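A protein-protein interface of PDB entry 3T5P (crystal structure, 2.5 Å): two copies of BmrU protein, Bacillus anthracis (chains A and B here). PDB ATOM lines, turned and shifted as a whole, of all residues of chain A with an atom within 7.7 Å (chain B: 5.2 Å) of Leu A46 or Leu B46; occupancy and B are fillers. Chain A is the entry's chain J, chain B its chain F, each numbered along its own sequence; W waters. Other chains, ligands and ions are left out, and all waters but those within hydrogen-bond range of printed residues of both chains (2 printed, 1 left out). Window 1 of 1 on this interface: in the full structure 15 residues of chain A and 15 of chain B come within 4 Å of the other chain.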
ATOM      1  N   GLU A  13      27.087   8.663   6.495  1.00  0.00           N
ATOM      2  CA  GLU A  13      26.292   8.210   7.633  1.00  0.00           C
ATOM      3  C   GLU A  13      25.993   9.368   8.624  1.00  0.00           C
ATOM      4  O   GLU A  13      24.861   9.506   9.117  1.00  0.00           O
ATOM      5  CB  GLU A  13      27.031   7.070   8.341  1.00  0.00           C
ATOM      6  CG  GLU A  13      26.178   6.270   9.339  1.00  0.00           C
ATOM      7  CD  GLU A  13      26.999   5.594  10.456  1.00  0.00           C
ATOM      8  OE1 GLU A  13      28.172   5.228  10.209  1.00  0.00           O
ATOM      9  OE2 GLU A  13      26.466   5.419  11.581  1.00  0.00           O
ATOM     10  N   LYS A  14      27.006  10.196   8.888  1.00  0.00           N
ATOM     11  CA  LYS A  14      26.904  11.306   9.835  1.00  0.00           C
ATOM     12  C   LYS A  14      27.380  12.584   9.212  1.00  0.00           C
ATOM     13  O   LYS A  14      28.408  12.600   8.566  1.00  0.00           O
ATOM     14  CB  LYS A  14      27.734  11.019  11.068  1.00  0.00           C
ATOM     15  CG  LYS A  14      27.224   9.849  11.842  1.00  0.00           C
ATOM     16  CD  LYS A  14      27.992   9.637  13.116  1.00  0.00           C
ATOM     17  CE  LYS A  14      27.523   8.371  13.819  1.00  0.00           C
ATOM     18  NZ  LYS A  14      28.036   8.269  15.202  1.00  0.00           N
ATOM     19  N   VAL A  15      26.617  13.647   9.393  1.00  0.00           N
ATOM     20  CA  VAL A  15      26.909  14.930   8.776  1.00  0.00           C
ATOM     21  C   VAL A  15      26.950  16.059   9.838  1.00  0.00           C
ATOM     22  O   VAL A  15      26.158  16.069  10.788  1.00  0.00           O
ATOM     23  CB  VAL A  15      25.830  15.285   7.717  1.00  0.00           C
ATOM     24  CG1 VAL A  15      26.116  16.640   7.077  1.00  0.00           C
ATOM     25  CG2 VAL A  15      25.743  14.206   6.655  1.00  0.00           C
ATOM     26  N   LEU A  16      27.885  16.987   9.660  1.00  0.00           N
ATOM     27  CA  LEU A  16      27.983  18.193  10.482  1.00  0.00           C
ATOM     28  C   LEU A  16      27.758  19.402   9.602  1.00  0.00           C
ATOM     29  O   LEU A  16      28.434  19.562   8.597  1.00  0.00           O
ATOM     30  CB  LEU A  16      29.361  18.308  11.151  1.00  0.00           C
ATOM     31  CG  LEU A  16      29.656  19.598  11.951  1.00  0.00           C
ATOM     32  CD1 LEU A  16      28.892  19.644  13.245  1.00  0.00           C
ATOM     33  CD2 LEU A  16      31.118  19.722  12.227  1.00  0.00           C
ATOM     34  N   LEU A  17      26.837  20.273   9.993  1.00  0.00           N
ATOM     35  CA  LEU A  17      26.658  21.557   9.335  1.00  0.00           C
ATOM     36  C   LEU A  17      27.143  22.669  10.280  1.00  0.00           C
ATOM     37  O   LEU A  17      26.638  22.811  11.391  1.00  0.00           O
ATOM     38  CB  LEU A  17      25.198  21.767   8.988  1.00  0.00           C
ATOM     39  CG  LEU A  17      24.789  23.166   8.528  1.00  0.00           C
ATOM     40  CD1 LEU A  17      25.498  23.523   7.216  1.00  0.00           C
ATOM     41  CD2 LEU A  17      23.290  23.245   8.409  1.00  0.00           C
ATOM     42  N   ILE A  18      28.163  23.416   9.850  1.00  0.00           N
ATOM     43  CA  ILE A  18      28.704  24.511  10.627  1.00  0.00           C
ATOM     44  C   ILE A  18      28.082  25.765  10.053  1.00  0.00           C
ATOM     45  O   ILE A  18      28.232  26.058   8.863  1.00  0.00           O
ATOM     46  CB  ILE A  18      30.235  24.612  10.535  1.00  0.00           C
ATOM     47  CG1 ILE A  18      30.910  23.391  11.173  1.00  0.00           C
ATOM     48  CG2 ILE A  18      30.704  25.895  11.201  1.00  0.00           C
ATOM     49  CD1 ILE A  18      32.386  23.256  10.880  1.00  0.00           C
ATOM     50  N   ILE A  35      18.339  26.450   3.921  1.00  0.00           N
ATOM     51  CA  ILE A  35      19.392  25.422   3.852  1.00  0.00           C
ATOM     52  C   ILE A  35      19.193  24.192   4.711  1.00  0.00           C
ATOM     53  O   ILE A  35      19.691  23.144   4.398  1.00  0.00           O
ATOM     54  CB  ILE A  35      20.811  26.002   4.105  1.00  0.00           C
ATOM     55  CG1 ILE A  35      21.072  26.241   5.572  1.00  0.00           C
ATOM     56  CG2 ILE A  35      21.023  27.309   3.341  1.00  0.00           C
ATOM     57  CD1 ILE A  35      22.426  26.893   5.816  1.00  0.00           C
ATOM     58  N   VAL A  36      18.475  24.289   5.805  1.00  0.00           N
ATOM     59  CA  VAL A  36      18.440  23.142   6.718  1.00  0.00           C
ATOM     60  C   VAL A  36      17.482  22.017   6.293  1.00  0.00           C
ATOM     61  O   VAL A  36      17.894  20.853   6.226  1.00  0.00           O
ATOM     62  CB  VAL A  36      18.223  23.559   8.198  1.00  0.00           C
ATOM     63  CG1 VAL A  36      18.226  22.336   9.100  1.00  0.00           C
ATOM     64  CG2 VAL A  36      19.332  24.498   8.644  1.00  0.00           C
ATOM     65  N   PRO A  37      16.219  22.345   5.995  1.00  0.00           N
ATOM     66  CA  PRO A  37      15.255  21.294   5.650  1.00  0.00           C
ATOM     67  C   PRO A  37      15.693  20.291   4.567  1.00  0.00           C
ATOM     68  O   PRO A  37      15.508  19.098   4.746  1.00  0.00           O
ATOM     69  CB  PRO A  37      14.041  22.084   5.188  1.00  0.00           C
ATOM     70  CG  PRO A  37      14.170  23.379   5.896  1.00  0.00           C
ATOM     71  CD  PRO A  37      15.606  23.679   5.916  1.00  0.00           C
ATOM     72  N   PRO A  38      16.284  20.761   3.466  1.00  0.00           N
ATOM     73  CA  PRO A  38      16.755  19.770   2.492  1.00  0.00           C
ATOM     74  C   PRO A  38      17.806  18.858   3.068  1.00  0.00           C
ATOM     75  O   PRO A  38      17.814  17.675   2.788  1.00  0.00           O
ATOM     76  CB  PRO A  38      17.355  20.614   1.362  1.00  0.00           C
ATOM     77  CG  PRO A  38      16.913  22.007   1.605  1.00  0.00           C
ATOM     78  CD  PRO A  38      16.576  22.140   3.048  1.00  0.00           C
ATOM     79  N   LEU A  39      18.685  19.409   3.891  1.00  0.00           N
ATOM     80  CA  LEU A  39      19.760  18.622   4.511  1.00  0.00           C
ATOM     81  C   LEU A  39      19.199  17.663   5.538  1.00  0.00           C
ATOM     82  O   LEU A  39      19.555  16.489   5.562  1.00  0.00           O
ATOM     83  CB  LEU A  39      20.800  19.531   5.141  1.00  0.00           C
ATOM     84  CG  LEU A  39      21.537  20.467   4.176  1.00  0.00           C
ATOM     85  CD1 LEU A  39      22.429  21.456   4.911  1.00  0.00           C
ATOM     86  CD2 LEU A  39      22.343  19.659   3.151  1.00  0.00           C
ATOM     87  N   ALA A  40      18.286  18.155   6.351  1.00  0.00           N
ATOM     88  CA  ALA A  40      17.653  17.320   7.371  1.00  0.00           C
ATOM     89  C   ALA A  40      16.823  16.182   6.765  1.00  0.00           C
ATOM     90  O   ALA A  40      16.787  15.075   7.308  1.00  0.00           O
ATOM     91  CB  ALA A  40      16.785  18.163   8.285  1.00  0.00           C
ATOM     92  N   ALA A  41      16.165  16.458   5.641  1.00  0.00           N
ATOM     93  CA  ALA A  41      15.370  15.428   4.919  1.00  0.00           C
ATOM     94  C   ALA A  41      16.274  14.334   4.349  1.00  0.00           C
ATOM     95  O   ALA A  41      15.955  13.168   4.452  1.00  0.00           O
ATOM     96  CB  ALA A  41      14.527  16.053   3.808  1.00  0.00           C
ATOM     97  N   ALA A  42      17.403  14.727   3.780  1.00  0.00           N
ATOM     98  CA  ALA A  42      18.316  13.799   3.132  1.00  0.00           C
ATOM     99  C   ALA A  42      19.193  12.992   4.103  1.00  0.00           C
ATOM    100  O   ALA A  42      19.560  11.858   3.823  1.00  0.00           O
ATOM    101  CB  ALA A  42      19.212  14.561   2.185  1.00  0.00           C
ATOM    102  N   PHE A  43      19.570  13.602   5.218  1.00  0.00           N
ATOM    103  CA  PHE A  43      20.593  13.033   6.104  1.00  0.00           C
ATOM    104  C   PHE A  43      20.011  12.764   7.488  1.00  0.00           C
ATOM    105  O   PHE A  43      19.787  13.683   8.274  1.00  0.00           O
ATOM    106  CB  PHE A  43      21.802  13.967   6.215  1.00  0.00           C
ATOM    107  CG  PHE A  43      22.471  14.264   4.905  1.00  0.00           C
ATOM    108  CD1 PHE A  43      23.014  13.251   4.138  1.00  0.00           C
ATOM    109  CD2 PHE A  43      22.560  15.565   4.442  1.00  0.00           C
ATOM    110  CE1 PHE A  43      23.631  13.532   2.943  1.00  0.00           C
ATOM    111  CE2 PHE A  43      23.174  15.858   3.247  1.00  0.00           C
ATOM    112  CZ  PHE A  43      23.719  14.843   2.496  1.00  0.00           C
ATOM    113  N   PRO A  44      19.773  11.495   7.800  1.00  0.00           N
ATOM    114  CA  PRO A  44      19.063  11.183   9.034  1.00  0.00           C
ATOM    115  C   PRO A  44      19.892  11.304  10.327  1.00  0.00           C
ATOM    116  O   PRO A  44      19.366  11.054  11.410  1.00  0.00           O
ATOM    117  CB  PRO A  44      18.617   9.734   8.810  1.00  0.00           C
ATOM    118  CG  PRO A  44      19.651   9.164   7.906  1.00  0.00           C
ATOM    119  CD  PRO A  44      20.093  10.290   7.020  1.00  0.00           C
ATOM    120  N   ASP A  45      21.171  11.649  10.206  1.00  0.00           N
ATOM    121  CA  ASP A  45      22.000  12.010  11.367  1.00  0.00           C
ATOM    122  C   ASP A  45      22.735  13.303  11.061  1.00  0.00           C
ATOM    123  O   ASP A  45      23.816  13.273  10.455  1.00  0.00           O
ATOM    124  CB  ASP A  45      22.982  10.892  11.703  1.00  0.00           C
ATOM    125  CG  ASP A  45      23.753  11.137  13.025  1.00  0.00           C
ATOM    126  OD1 ASP A  45      23.976  12.315  13.393  1.00  0.00           O
ATOM    127  OD2 ASP A  45      24.131  10.130  13.688  1.00  0.00           O
ATOM    128  N   LEU A  46      22.141  14.422  11.475  1.00  0.00           N
ATOM    129  CA  LEU A  46      22.646  15.764  11.145  1.00  0.00           C
ATOM    130  C   LEU A  46      22.856  16.586  12.424  1.00  0.00           C
ATOM    131  O   LEU A  46      21.972  16.705  13.261  1.00  0.00           O
ATOM    132  CB  LEU A  46      21.666  16.487  10.224  1.00  0.00           C
ATOM    133  CG  LEU A  46      22.007  17.905   9.769  1.00  0.00           C
ATOM    134  CD1 LEU A  46      23.313  17.970   8.984  1.00  0.00           C
ATOM    135  CD2 LEU A  46      20.876  18.466   8.963  1.00  0.00           C
ATOM    136  N   HIS A  47      24.049  17.137  12.564  1.00  0.00           N
ATOM    137  CA  HIS A  47      24.418  17.912  13.696  1.00  0.00           C
ATOM    138  C   HIS A  47      24.694  19.310  13.203  1.00  0.00           C
ATOM    139  O   HIS A  47      25.490  19.486  12.299  1.00  0.00           O
ATOM    140  CB  HIS A  47      25.678  17.319  14.326  1.00  0.00           C
ATOM    141  CG  HIS A  47      25.884  17.711  15.761  1.00  0.00           C
ATOM    142  ND1 HIS A  47      26.551  16.917  16.659  1.00  0.00           N
ATOM    143  CD2 HIS A  47      25.469  18.793  16.458  1.00  0.00           C
ATOM    144  CE1 HIS A  47      26.546  17.499  17.849  1.00  0.00           C
ATOM    145  NE2 HIS A  47      25.898  18.641  17.753  1.00  0.00           N
ATOM    146  N   ILE A  48      24.046  20.299  13.811  1.00  0.00           N
ATOM    147  CA  ILE A  48      24.194  21.698  13.430  1.00  0.00           C
ATOM    148  C   ILE A  48      24.844  22.500  14.592  1.00  0.00           C
ATOM    149  O   ILE A  48      24.309  22.574  15.692  1.00  0.00           O
ATOM    150  CB  ILE A  48      22.864  22.318  13.061  1.00  0.00           C
ATOM    151  CG1 ILE A  48      22.103  21.402  12.113  1.00  0.00           C
ATOM    152  CG2 ILE A  48      23.087  23.685  12.443  1.00  0.00           C
ATOM    153  CD1 ILE A  48      20.678  21.865  11.795  1.00  0.00           C
ATOM    154  N   LEU A  49      25.995  23.100  14.305  1.00  0.00           N
ATOM    155  CA  LEU A  49      26.716  23.902  15.261  1.00  0.00           C
ATOM    156  C   LEU A  49      26.841  25.319  14.723  1.00  0.00           C
ATOM    157  O   LEU A  49      27.300  25.516  13.628  1.00  0.00           O
ATOM    158  CB  LEU A  49      28.107  23.326  15.520  1.00  0.00           C
ATOM    159  CG  LEU A  49      28.211  22.017  16.297  1.00  0.00           C
ATOM    160  CD1 LEU A  49      29.656  21.528  16.371  1.00  0.00           C
ATOM    161  CD2 LEU A  49      27.590  22.165  17.713  1.00  0.00           C
ATOM    162  N   HIS A  50      26.440  26.308  15.504  1.00  0.00           N
ATOM    163  CA  HIS A  50      26.753  27.708  15.176  1.00  0.00           C
ATOM    164  C   HIS A  50      28.134  28.108  15.699  1.00  0.00           C
ATOM    165  O   HIS A  50      28.522  27.736  16.810  1.00  0.00           O
ATOM    166  CB  HIS A  50      25.766  28.651  15.815  1.00  0.00           C
ATOM    167  CG  HIS A  50      24.361  28.411  15.408  1.00  0.00           C
ATOM    168  ND1 HIS A  50      23.343  29.264  15.757  1.00  0.00           N
ATOM    169  CD2 HIS A  50      23.793  27.406  14.703  1.00  0.00           C
ATOM    170  CE1 HIS A  50      22.207  28.792  15.280  1.00  0.00           C
ATOM    171  NE2 HIS A  50      22.454  27.669  14.629  1.00  0.00           N
ATOM    172  N   VAL A  68      32.563  12.124  11.990  1.00  0.00           N
ATOM    173  CA  VAL A  68      31.583  12.561  11.013  1.00  0.00           C
ATOM    174  C   VAL A  68      32.107  12.286   9.616  1.00  0.00           C
ATOM    175  O   VAL A  68      33.303  12.169   9.423  1.00  0.00           O
ATOM    176  CB  VAL A  68      31.240  14.055  11.291  1.00  0.00           C
ATOM    177  CG1 VAL A  68      31.529  14.956  10.151  1.00  0.00           C
ATOM    178  CG2 VAL A  68      29.821  14.163  11.790  1.00  0.00           C
ATOM    179  N   LEU A  70      30.753  13.835   6.616  1.00  0.00           N
ATOM    180  CA  LEU A  70      30.641  15.031   5.795  1.00  0.00           C
ATOM    181  C   LEU A  70      30.596  16.245   6.712  1.00  0.00           C
ATOM    182  O   LEU A  70      29.929  16.200   7.732  1.00  0.00           O
ATOM    183  CB  LEU A  70      29.381  14.969   4.947  1.00  0.00           C
ATOM    184  CG  LEU A  70      29.029  16.188   4.073  1.00  0.00           C
ATOM    185  CD1 LEU A  70      30.141  16.510   3.066  1.00  0.00           C
ATOM    186  CD2 LEU A  70      27.685  15.968   3.376  1.00  0.00           C
ATOM    187  N   ILE A  72      29.683  20.281   6.317  1.00  0.00           N
ATOM    188  CA  ILE A  72      29.186  21.354   5.476  1.00  0.00           C
ATOM    189  C   ILE A  72      29.451  22.679   6.159  1.00  0.00           C
ATOM    190  O   ILE A  72      29.103  22.844   7.313  1.00  0.00           O
ATOM    191  CB  ILE A  72      27.665  21.228   5.242  1.00  0.00           C
ATOM    192  CG1 ILE A  72      27.295  19.843   4.726  1.00  0.00           C
ATOM    193  CG2 ILE A  72      27.196  22.292   4.260  1.00  0.00           C
ATOM    194  CD1 ILE A  72      25.815  19.557   4.825  1.00  0.00           C
ATOM    195  N   VAL B  15      21.004  20.261  22.300  1.00  0.00           N
ATOM    196  CA  VAL B  15      19.655  19.776  22.028  1.00  0.00           C
ATOM    197  C   VAL B  15      19.657  18.590  21.043  1.00  0.00           C
ATOM    198  O   VAL B  15      20.433  18.555  20.102  1.00  0.00           O
ATOM    199  CB  VAL B  15      18.775  20.918  21.468  1.00  0.00           C
ATOM    200  CG1 VAL B  15      17.353  20.434  21.185  1.00  0.00           C
ATOM    201  CG2 VAL B  15      18.779  22.102  22.428  1.00  0.00           C
ATOM    202  N   LEU B  16      18.784  17.622  21.300  1.00  0.00           N
ATOM    203  CA  LEU B  16      18.540  16.491  20.396  1.00  0.00           C
ATOM    204  C   LEU B  16      17.103  16.551  19.886  1.00  0.00           C
ATOM    205  O   LEU B  16      16.159  16.656  20.689  1.00  0.00           O
ATOM    206  CB  LEU B  16      18.749  15.150  21.111  1.00  0.00           C
ATOM    207  CG  LEU B  16      18.384  13.895  20.278  1.00  0.00           C
ATOM    208  CD1 LEU B  16      19.403  13.704  19.176  1.00  0.00           C
ATOM    209  CD2 LEU B  16      18.310  12.665  21.126  1.00  0.00           C
ATOM    210  N   LEU B  17      16.936  16.475  18.571  1.00  0.00           N
ATOM    211  CA  LEU B  17      15.604  16.371  17.971  1.00  0.00           C
ATOM    212  C   LEU B  17      15.470  14.993  17.382  1.00  0.00           C
ATOM    213  O   LEU B  17      16.257  14.591  16.506  1.00  0.00           O
ATOM    214  CB  LEU B  17      15.377  17.444  16.912  1.00  0.00           C
ATOM    215  CG  LEU B  17      14.149  17.341  16.018  1.00  0.00           C
ATOM    216  CD1 LEU B  17      12.819  17.408  16.814  1.00  0.00           C
ATOM    217  CD2 LEU B  17      14.203  18.418  14.934  1.00  0.00           C
ATOM    218  N   VAL B  36      12.178  22.593  11.931  1.00  0.00           N
ATOM    219  CA  VAL B  36      13.626  22.666  12.171  1.00  0.00           C
ATOM    220  C   VAL B  36      14.184  24.097  12.241  1.00  0.00           C
ATOM    221  O   VAL B  36      14.916  24.419  13.147  1.00  0.00           O
ATOM    222  CB  VAL B  36      14.443  21.812  11.183  1.00  0.00           C
ATOM    223  CG1 VAL B  36      15.926  21.913  11.532  1.00  0.00           C
ATOM    224  CG2 VAL B  36      14.000  20.337  11.257  1.00  0.00           C
ATOM    225  N   LEU B  39      14.047  25.898  15.565  1.00  0.00           N
ATOM    226  CA  LEU B  39      14.896  25.217  16.527  1.00  0.00           C
ATOM    227  C   LEU B  39      16.368  25.486  16.238  1.00  0.00           C
ATOM    228  O   LEU B  39      17.144  25.789  17.140  1.00  0.00           O
ATOM    229  CB  LEU B  39      14.620  23.717  16.530  1.00  0.00           C
ATOM    230  CG  LEU B  39      13.190  23.304  16.946  1.00  0.00           C
ATOM    231  CD1 LEU B  39      12.977  21.818  16.776  1.00  0.00           C
ATOM    232  CD2 LEU B  39      12.899  23.728  18.345  1.00  0.00           C
ATOM    233  N   ALA B  40      16.745  25.387  14.969  1.00  0.00           N
ATOM    234  CA  ALA B  40      18.121  25.611  14.561  1.00  0.00           C
ATOM    235  C   ALA B  40      18.565  27.040  14.824  1.00  0.00           C
ATOM    236  O   ALA B  40      19.717  27.254  15.115  1.00  0.00           O
ATOM    237  CB  ALA B  40      18.301  25.273  13.126  1.00  0.00           C
ATOM    238  N   PHE B  43      18.841  27.346  18.887  1.00  0.00           N
ATOM    239  CA  PHE B  43      19.747  26.419  19.610  1.00  0.00           C
ATOM    240  C   PHE B  43      20.997  26.150  18.816  1.00  0.00           C
ATOM    241  O   PHE B  43      20.981  25.408  17.867  1.00  0.00           O
ATOM    242  CB  PHE B  43      19.054  25.095  19.919  1.00  0.00           C
ATOM    243  CG  PHE B  43      17.822  25.236  20.756  1.00  0.00           C
ATOM    244  CD1 PHE B  43      17.879  25.810  22.000  1.00  0.00           C
ATOM    245  CD2 PHE B  43      16.590  24.780  20.283  1.00  0.00           C
ATOM    246  CE1 PHE B  43      16.725  25.928  22.782  1.00  0.00           C
ATOM    247  CE2 PHE B  43      15.443  24.892  21.056  1.00  0.00           C
ATOM    248  CZ  PHE B  43      15.507  25.469  22.302  1.00  0.00           C
ATOM    249  N   PRO B  44      22.110  26.731  19.223  1.00  0.00           N
ATOM    250  CA  PRO B  44      23.302  26.639  18.395  1.00  0.00           C
ATOM    251  C   PRO B  44      24.030  25.287  18.405  1.00  0.00           C
ATOM    252  O   PRO B  44      25.037  25.112  17.688  1.00  0.00           O
ATOM    253  CB  PRO B  44      24.196  27.752  18.971  1.00  0.00           C
ATOM    254  CG  PRO B  44      23.785  27.853  20.391  1.00  0.00           C
ATOM    255  CD  PRO B  44      22.321  27.541  20.432  1.00  0.00           C
ATOM    256  N   ASP B  45      23.554  24.343  19.199  1.00  0.00           N
ATOM    257  CA  ASP B  45      24.054  22.973  19.153  1.00  0.00           C
ATOM    258  C   ASP B  45      22.861  22.029  19.069  1.00  0.00           C
ATOM    259  O   ASP B  45      22.314  21.613  20.088  1.00  0.00           O
ATOM    260  CB  ASP B  45      24.923  22.645  20.372  1.00  0.00           C
ATOM    261  CG  ASP B  45      25.589  21.245  20.281  1.00  0.00           C
ATOM    262  OD1 ASP B  45      24.992  20.304  19.665  1.00  0.00           O
ATOM    263  OD2 ASP B  45      26.743  21.105  20.819  1.00  0.00           O
ATOM    264  N   LEU B  46      22.488  21.666  17.848  1.00  0.00           N
ATOM    265  CA  LEU B  46      21.287  20.874  17.582  1.00  0.00           C
ATOM    266  C   LEU B  46      21.618  19.631  16.789  1.00  0.00           C
ATOM    267  O   LEU B  46      22.229  19.710  15.745  1.00  0.00           O
ATOM    268  CB  LEU B  46      20.263  21.710  16.827  1.00  0.00           C
ATOM    269  CG  LEU B  46      18.930  21.056  16.442  1.00  0.00           C
ATOM    270  CD1 LEU B  46      18.092  20.544  17.625  1.00  0.00           C
ATOM    271  CD2 LEU B  46      18.139  22.078  15.595  1.00  0.00           C
ATOM    272  N   HIS B  47      21.219  18.482  17.322  1.00  0.00           N
ATOM    273  CA  HIS B  47      21.474  17.190  16.699  1.00  0.00           C
ATOM    274  C   HIS B  47      20.139  16.612  16.316  1.00  0.00           C
ATOM    275  O   HIS B  47      19.242  16.555  17.172  1.00  0.00           O
ATOM    276  CB  HIS B  47      22.149  16.257  17.682  1.00  0.00           C
ATOM    277  CG  HIS B  47      22.887  15.114  17.042  1.00  0.00           C
ATOM    278  ND1 HIS B  47      23.935  14.479  17.652  1.00  0.00           N
ATOM    279  CD2 HIS B  47      22.748  14.518  15.838  1.00  0.00           C
ATOM    280  CE1 HIS B  47      24.415  13.543  16.860  1.00  0.00           C
ATOM    281  NE2 HIS B  47      23.709  13.543  15.747  1.00  0.00           N
ATOM    282  N   ILE B  48      19.992  16.206  15.043  1.00  0.00           N
ATOM    283  CA  ILE B  48      18.727  15.683  14.501  1.00  0.00           C
ATOM    284  C   ILE B  48      18.906  14.246  14.064  1.00  0.00           C
ATOM    285  O   ILE B  48      19.721  13.945  13.196  1.00  0.00           O
ATOM    286  CB  ILE B  48      18.242  16.509  13.297  1.00  0.00           C
ATOM    287  CG1 ILE B  48      18.251  17.997  13.658  1.00  0.00           C
ATOM    288  CG2 ILE B  48      16.843  16.110  12.905  1.00  0.00           C
ATOM    289  CD1 ILE B  48      17.858  18.882  12.538  1.00  0.00           C
ATOM    290  N   ILE B  72      13.847  16.764  22.137  1.00  0.00           N
ATOM    291  CA  ILE B  72      12.569  17.052  21.497  1.00  0.00           C
ATOM    292  C   ILE B  72      12.164  15.829  20.659  1.00  0.00           C
ATOM    293  O   ILE B  72      12.968  15.329  19.872  1.00  0.00           O
ATOM    294  CB  ILE B  72      12.668  18.232  20.539  1.00  0.00           C
ATOM    295  CG1 ILE B  72      13.289  19.436  21.238  1.00  0.00           C
ATOM    296  CG2 ILE B  72      11.285  18.554  19.956  1.00  0.00           C
ATOM    297  CD1 ILE B  72      13.850  20.516  20.270  1.00  0.00           C
HETATM  298  O   HOH W   1      18.500  14.720  10.495  1.00  0.00           O
HETATM  299  O   HOH W   2      27.788  25.888  18.800  1.00  0.00           O
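Val B36 touches its own counterpart, Val A36. Asp A45 touches Ile B48, and with the chains exchanged Ile A48 touches Asp B45. Leu A46 touches His B47, and with the chains exchanged His A47 touches Leu B46. His B47 touches its own counterpart, His A47.
Leu A46 touches just these residues of chain B: Leu B46, His B47 and Ile B48. Of the printed residues of chain A, Leu B46 touches Leu A46 (3.9 Å), His A47 (3.4 Å) and Ile A48 (2.7 Å). Of the printed residues of chain A, His B47 touches Asp A45 (2.7 Å), Leu A46 (3.5 Å) and His A47 (3.7 Å). Of the printed residues of chain A, Asp B45 touches His A47 (2.7 Å), Ile A48 (3.5 Å) and Leu A49 (3.4 Å). Of the printed residues of chain A, Pro B44 touches Ile A48, Leu A49 and His A50. Of the printed residues of chain A, Ile B48 touches Pro A44 (3.4 Å), Asp A45 (3.5 Å) and Leu A46 (2.7 Å). Leu A39 touches none of the printed residues of chain B. Val A15 touches none of the printed residues of chain B. The nearest printed residue of chain B that does not touch Leu A46 is Val B36 (6.6 Å). The nearest residue of chain A that does not touch Leu B46 is Leu A49 (5.1 Å). The nearest printed residue of chain B that does not touch His A50 is Phe B43 (4.2 Å).
Val A36 touches Val B36 (CG1 to CG1, 3.4 Å). Asp A45 touches Ile B48 (CA to O, 3.5 Å). Leu B46 touches Leu A46 (O to O, 3.9 Å). His B47 touches Leu A46. Leu B46 touches His A47. His A47 touches His B47 (ND1 to ND1, 3.7 Å). CA of Asp B45 touches O of Ile A48 (3.5 Å). Leu A49 touches Pro B44 (CA to O, 3.2 Å). Leu A49 touches Asp B45.
Water W1 lies within hydrogen-bond range of the backbone carbonyl oxygen (O) of Phe A43 (2.8 Å) and the backbone carbonyl oxygen (O) of Ile B48 (3.1 Å). Water W2 lies within hydrogen-bond range of O of His A50 (2.8 Å) and O of Pro B44 (3.1 Å).
The backbone carbonyl oxygen of Asp B45 sits at hydrogen-bond distance from the backbone NH of Val B15 (2.9 Å). The backbone NH (N) of His B47 is in hydrogen-bond range of the backbone carbonyl oxygen (O) of Val B15 (2.9 Å). N of Leu B17 lies within hydrogen-bond range of O of His B47 (2.7 Å). The backbone carbonyl oxygen (O) of Val A15 sits at hydrogen-bond distance from the backbone NH (N) of His A47. The backbone NH of Leu A17 is in hydrogen-bond range of the backbone carbonyl oxygen of His A47 (2.8 Å). O of Leu A17 sits at hydrogen-bond distance from N of Leu A49, 3.0 Å away.
O of Ala B40 sits at hydrogen-bond distance from NE2 of His A50 (2.8 Å). The backbone carbonyl oxygen (O) of Pro B44 is in hydrogen-bond range of the backbone NH (N) of His A50, 2.9 Å away. The side-chain carboxylate (OD1) of Asp B45 is in hydrogen-bond range of a ring nitrogen (NE2) of His A47, at 2.7 Å. The backbone carbonyl oxygen (O) of Leu B46 sits at hydrogen-bond distance from the backbone NH (N) of Ile A48. The side-chain carboxylate (OD1) of Asp A45 lies within hydrogen-bond range of a ring nitrogen (NE2) of His B47 (2.7 Å). The backbone NH (N) of Ile B48 sits at hydrogen-bond distance from the backbone carbonyl oxygen (O) of Leu A46. O of Pro A44 lies close to O of Ile B48 (3.4 Å). The backbone carbonyl oxygen (O) of Ile A48 sits close to the backbone carbonyl oxygen (O) of Pro B44 (3.3 Å).
Hydrophobic or aromatic side chains of chain B that line the printed part of chain A: Val B36, Pro B44, His B47 and Ile B48. Of the 25 printed residues of chain A, 8 touch a printed residue of chain B. Among the printed residues, no Asp or Glu carboxylate lies within 4 Å of a Lys or Arg side-chain nitrogen of the other chain.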
